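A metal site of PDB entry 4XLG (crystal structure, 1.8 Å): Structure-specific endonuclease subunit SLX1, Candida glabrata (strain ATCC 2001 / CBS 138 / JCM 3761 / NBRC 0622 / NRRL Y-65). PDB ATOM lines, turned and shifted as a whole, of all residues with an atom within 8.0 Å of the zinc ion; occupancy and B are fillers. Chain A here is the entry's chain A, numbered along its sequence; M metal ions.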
ATOM      1  N   PHE A 241      31.966 -11.095  -8.664  1.00  0.00           N
ATOM      2  CA  PHE A 241      31.648 -11.465 -10.038  1.00  0.00           C
ATOM      3  C   PHE A 241      30.194 -11.185 -10.324  1.00  0.00           C
ATOM      4  O   PHE A 241      29.352 -11.250  -9.422  1.00  0.00           O
ATOM      5  CB  PHE A 241      31.898 -12.963 -10.298  1.00  0.00           C
ATOM      6  CG  PHE A 241      33.295 -13.402  -9.985  1.00  0.00           C
ATOM      7  CD1 PHE A 241      33.660 -13.697  -8.673  1.00  0.00           C
ATOM      8  CD2 PHE A 241      34.229 -13.517 -10.993  1.00  0.00           C
ATOM      9  CE1 PHE A 241      34.946 -14.115  -8.396  1.00  0.00           C
ATOM     10  CE2 PHE A 241      35.524 -13.937 -10.720  1.00  0.00           C
ATOM     11  CZ  PHE A 241      35.875 -14.228  -9.417  1.00  0.00           C
ATOM     12  N   CYS A 242      29.862 -10.962 -11.587  1.00  0.00           N
ATOM     13  CA  CYS A 242      28.470 -10.879 -11.964  1.00  0.00           C
ATOM     14  C   CYS A 242      27.837 -12.267 -11.812  1.00  0.00           C
ATOM     15  O   CYS A 242      28.504 -13.293 -12.065  1.00  0.00           O
ATOM     16  CB  CYS A 242      28.313 -10.386 -13.401  1.00  0.00           C
ATOM     17  SG  CYS A 242      26.507 -10.198 -13.808  1.00  0.00           S
ATOM     18  N   ARG A 243      26.571 -12.306 -11.419  1.00  0.00           N
ATOM     19  CA  ARG A 243      25.855 -13.574 -11.324  1.00  0.00           C
ATOM     20  C   ARG A 243      25.686 -14.210 -12.691  1.00  0.00           C
ATOM     21  O   ARG A 243      25.504 -15.420 -12.780  1.00  0.00           O
ATOM     22  CB  ARG A 243      24.501 -13.399 -10.649  1.00  0.00           C
ATOM     23  CG  ARG A 243      23.456 -12.678 -11.498  1.00  0.00           C
ATOM     24  CD  ARG A 243      22.119 -12.785 -10.759  1.00  0.00           C
ATOM     25  NE  ARG A 243      21.027 -12.009 -11.353  1.00  0.00           N
ATOM     26  CZ  ARG A 243      20.161 -12.494 -12.247  1.00  0.00           C
ATOM     27  NH1 ARG A 243      20.263 -13.759 -12.655  1.00  0.00           N
ATOM     28  NH2 ARG A 243      19.188 -11.716 -12.717  1.00  0.00           N
ATOM     29  N   ASP A 244      25.717 -13.413 -13.749  1.00  0.00           N
ATOM     30  CA  ASP A 244      25.700 -13.958 -15.101  1.00  0.00           C
ATOM     31  C   ASP A 244      27.146 -14.364 -15.452  1.00  0.00           C
ATOM     32  O   ASP A 244      28.003 -13.509 -15.684  1.00  0.00           O
ATOM     33  CB  ASP A 244      25.153 -12.910 -16.085  1.00  0.00           C
ATOM     34  CG  ASP A 244      25.148 -13.387 -17.537  1.00  0.00           C
ATOM     35  OD1 ASP A 244      25.735 -14.438 -17.865  1.00  0.00           O
ATOM     36  OD2 ASP A 244      24.557 -12.662 -18.379  1.00  0.00           O
ATOM     37  N   THR A 245      27.419 -15.677 -15.496  1.00  0.00           N
ATOM     38  CA  THR A 245      28.789 -16.167 -15.687  1.00  0.00           C
ATOM     39  C   THR A 245      29.342 -15.838 -17.076  1.00  0.00           C
ATOM     40  O   THR A 245      30.537 -16.006 -17.331  1.00  0.00           O
ATOM     41  CB  THR A 245      28.887 -17.704 -15.469  1.00  0.00           C
ATOM     42  OG1 THR A 245      28.033 -18.369 -16.399  1.00  0.00           O
ATOM     43  CG2 THR A 245      28.507 -18.112 -14.033  1.00  0.00           C
ATOM     44  N   SER A 246      28.487 -15.404 -17.994  1.00  0.00           N
ATOM     45  CA  SER A 246      28.991 -15.022 -19.313  1.00  0.00           C
ATOM     46  C   SER A 246      29.213 -13.502 -19.367  1.00  0.00           C
ATOM     47  O   SER A 246      29.826 -12.991 -20.299  1.00  0.00           O
ATOM     48  CB  SER A 246      28.054 -15.485 -20.431  1.00  0.00           C
ATOM     49  OG  SER A 246      26.803 -14.837 -20.299  1.00  0.00           O
ATOM     50  N   CYS A 247      28.725 -12.782 -18.358  1.00  0.00           N
ATOM     51  CA  CYS A 247      29.077 -11.365 -18.230  1.00  0.00           C
ATOM     52  C   CYS A 247      30.516 -11.297 -17.745  1.00  0.00           C
ATOM     53  O   CYS A 247      30.961 -12.131 -16.947  1.00  0.00           O
ATOM     54  CB  CYS A 247      28.138 -10.622 -17.278  1.00  0.00           C
ATOM     55  SG  CYS A 247      28.621  -8.871 -16.966  1.00  0.00           S
ATOM     56  N   THR A 248      31.246 -10.295 -18.222  1.00  0.00           N
ATOM     57  CA  THR A 248      32.649 -10.207 -17.882  1.00  0.00           C
ATOM     58  C   THR A 248      32.951  -9.349 -16.644  1.00  0.00           C
ATOM     59  O   THR A 248      34.111  -9.195 -16.303  1.00  0.00           O
ATOM     60  CB  THR A 248      33.460  -9.631 -19.064  1.00  0.00           C
ATOM     61  OG1 THR A 248      32.971  -8.306 -19.375  1.00  0.00           O
ATOM     62  CG2 THR A 248      33.326 -10.527 -20.283  1.00  0.00           C
ATOM     63  N   PHE A 249      31.935  -8.799 -15.983  1.00  0.00           N
ATOM     64  CA  PHE A 249      32.205  -7.980 -14.780  1.00  0.00           C
ATOM     65  C   PHE A 249      32.927  -8.786 -13.704  1.00  0.00           C
ATOM     66  O   PHE A 249      32.445  -9.834 -13.220  1.00  0.00           O
ATOM     67  CB  PHE A 249      30.911  -7.414 -14.183  1.00  0.00           C
ATOM     68  CG  PHE A 249      31.114  -6.806 -12.828  1.00  0.00           C
ATOM     69  CD1 PHE A 249      31.961  -5.718 -12.657  1.00  0.00           C
ATOM     70  CD2 PHE A 249      30.470  -7.328 -11.709  1.00  0.00           C
ATOM     71  CE1 PHE A 249      32.164  -5.156 -11.390  1.00  0.00           C
ATOM     72  CE2 PHE A 249      30.646  -6.766 -10.454  1.00  0.00           C
ATOM     73  CZ  PHE A 249      31.510  -5.673 -10.296  1.00  0.00           C
ATOM     74  N   VAL A 250      34.100  -8.282 -13.331  1.00  0.00           N
ATOM     75  CA  VAL A 250      34.848  -8.837 -12.211  1.00  0.00           C
ATOM     76  C   VAL A 250      35.530  -7.672 -11.477  1.00  0.00           C
ATOM     77  O   VAL A 250      35.962  -6.724 -12.118  1.00  0.00           O
ATOM     78  CB  VAL A 250      35.879  -9.897 -12.679  1.00  0.00           C
ATOM     79  CG1 VAL A 250      36.851  -9.311 -13.697  1.00  0.00           C
ATOM     80  CG2 VAL A 250      36.601 -10.532 -11.512  1.00  0.00           C
ATOM     81  N   LYS A 278      23.363  -3.339  -8.679  1.00  0.00           N
ATOM     82  CA  LYS A 278      23.311  -3.823 -10.059  1.00  0.00           C
ATOM     83  C   LYS A 278      24.701  -3.941 -10.620  1.00  0.00           C
ATOM     84  O   LYS A 278      25.567  -3.113 -10.334  1.00  0.00           O
ATOM     85  CB  LYS A 278      22.457  -2.898 -10.948  1.00  0.00           C
ATOM     86  CG  LYS A 278      21.001  -2.821 -10.525  1.00  0.00           C
ATOM     87  N   CYS A 279      24.911  -4.946 -11.456  1.00  0.00           N
ATOM     88  CA  CYS A 279      26.170  -5.082 -12.163  1.00  0.00           C
ATOM     89  C   CYS A 279      26.456  -3.810 -12.979  1.00  0.00           C
ATOM     90  O   CYS A 279      25.630  -3.377 -13.776  1.00  0.00           O
ATOM     91  CB  CYS A 279      26.148  -6.304 -13.079  1.00  0.00           C
ATOM     92  SG  CYS A 279      27.614  -6.433 -14.122  1.00  0.00           S
ATOM     93  N   PRO A 280      27.640  -3.211 -12.791  1.00  0.00           N
ATOM     94  CA  PRO A 280      27.976  -2.001 -13.547  1.00  0.00           C
ATOM     95  C   PRO A 280      28.092  -2.226 -15.061  1.00  0.00           C
ATOM     96  O   PRO A 280      28.141  -1.255 -15.809  1.00  0.00           O
ATOM     97  CB  PRO A 280      29.330  -1.579 -12.952  1.00  0.00           C
ATOM     98  CG  PRO A 280      29.924  -2.844 -12.445  1.00  0.00           C
ATOM     99  CD  PRO A 280      28.735  -3.621 -11.886  1.00  0.00           C
ATOM    100  N   LYS A 281      28.129  -3.481 -15.495  1.00  0.00           N
ATOM    101  CA  LYS A 281      28.287  -3.770 -16.916  1.00  0.00           C
ATOM    102  C   LYS A 281      26.954  -4.082 -17.604  1.00  0.00           C
ATOM    103  O   LYS A 281      26.606  -3.459 -18.611  1.00  0.00           O
ATOM    104  CB  LYS A 281      29.254  -4.929 -17.139  1.00  0.00           C
ATOM    105  CG  LYS A 281      30.694  -4.624 -16.790  1.00  0.00           C
ATOM    106  CD  LYS A 281      31.667  -5.223 -17.841  1.00  0.00           C
ATOM    107  N   CYS A 282      26.210  -5.037 -17.073  1.00  0.00           N
ATOM    108  CA  CYS A 282      25.010  -5.517 -17.749  1.00  0.00           C
ATOM    109  C   CYS A 282      23.749  -5.057 -17.010  1.00  0.00           C
ATOM    110  O   CYS A 282      22.634  -5.268 -17.482  1.00  0.00           O
ATOM    111  CB  CYS A 282      25.023  -7.043 -17.859  1.00  0.00           C
ATOM    112  SG  CYS A 282      24.603  -7.854 -16.293  1.00  0.00           S
ATOM    113  N   TYR A 283      23.943  -4.467 -15.826  1.00  0.00           N
ATOM    114  CA  TYR A 283      22.875  -3.810 -15.067  1.00  0.00           C
ATOM    115  C   TYR A 283      21.930  -4.791 -14.407  1.00  0.00           C
ATOM    116  O   TYR A 283      20.929  -4.385 -13.838  1.00  0.00           O
ATOM    117  CB  TYR A 283      22.087  -2.838 -15.971  1.00  0.00           C
ATOM    118  N   THR A 284      22.262  -6.072 -14.452  1.00  0.00           N
ATOM    119  CA  THR A 284      21.407  -7.063 -13.808  1.00  0.00           C
ATOM    120  C   THR A 284      21.484  -6.945 -12.292  1.00  0.00           C
ATOM    121  O   THR A 284      22.488  -6.542 -11.711  1.00  0.00           O
ATOM    122  CB  THR A 284      21.746  -8.506 -14.239  1.00  0.00           C
ATOM    123  OG1 THR A 284      20.652  -9.359 -13.920  1.00  0.00           O
ATOM    124  CG2 THR A 284      22.992  -9.004 -13.514  1.00  0.00           C
ATOM    125  N   LEU A 285      20.379  -7.277 -11.647  1.00  0.00           N
ATOM    126  CA  LEU A 285      20.289  -7.215 -10.216  1.00  0.00           C
ATOM    127  C   LEU A 285      21.106  -8.321  -9.554  1.00  0.00           C
ATOM    128  O   LEU A 285      20.939  -9.504  -9.876  1.00  0.00           O
ATOM    129  CB  LEU A 285      18.840  -7.337  -9.785  1.00  0.00           C
ATOM    130  CG  LEU A 285      18.613  -6.851  -8.364  1.00  0.00           C
ATOM    131  CD1 LEU A 285      18.400  -5.343  -8.457  1.00  0.00           C
ATOM    132  CD2 LEU A 285      17.409  -7.569  -7.786  1.00  0.00           C
ATOM    133  N   LEU A 286      21.969  -7.949  -8.628  1.00  0.00           N
ATOM    134  CA  LEU A 286      22.768  -8.929  -7.900  1.00  0.00           C
ATOM    135  C   LEU A 286      22.225  -9.152  -6.500  1.00  0.00           C
ATOM    136  O   LEU A 286      21.600  -8.266  -5.920  1.00  0.00           O
ATOM    137  CB  LEU A 286      24.222  -8.458  -7.832  1.00  0.00           C
ATOM    138  CG  LEU A 286      24.861  -8.081  -9.167  1.00  0.00           C
ATOM    139  CD1 LEU A 286      26.231  -7.511  -8.896  1.00  0.00           C
ATOM    140  CD2 LEU A 286      24.968  -9.319 -10.059  1.00  0.00           C
HETATM  141 ZN    ZN M   1      26.845  -8.356 -15.374  1.00  0.00          ZN
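N of Cys 279 lies within hydrogen-bond range of O of Thr 284, 2.9 Å away.
The side-chain sulfur of Cys 279 lies close to the backbone NH of Lys 281 (3.3 Å).
SG of Cys 247 lies close to N of Phe 249, at 3.5 Å.
N of Cys 247 sits at hydrogen-bond distance from OD1 of Asp 244.
The backbone NH (N) of Cys 242 lies within hydrogen-bond range of the backbone carbonyl oxygen (O) of Phe 249 (3.3 Å).
The side-chain sulfur (SG) of Cys 242 lies close to the backbone NH (N) of Asp 244 (3.3 Å).
The backbone NH of Thr 284 lies close to the side-chain sulfur of Cys 282 (3.5 Å).
Of the 19 residues printed, 4 come within 4 Å of the zinc ion.
Along chain A the residues within 4 Å of the zinc ion span positions 242 to 282.
The zinc ion is bound by SG of Cys 279 (2.4 Å).
The zinc ion is bound by the side-chain sulfur (SG) of Cys 247 (2.4 Å).
SG of Cys 242 binds the zinc ion (2.4 Å).
The zinc ion is bound by SG of Cys 282, at 2.5 Å.
The zinc ion has four donor atoms within binding distance.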
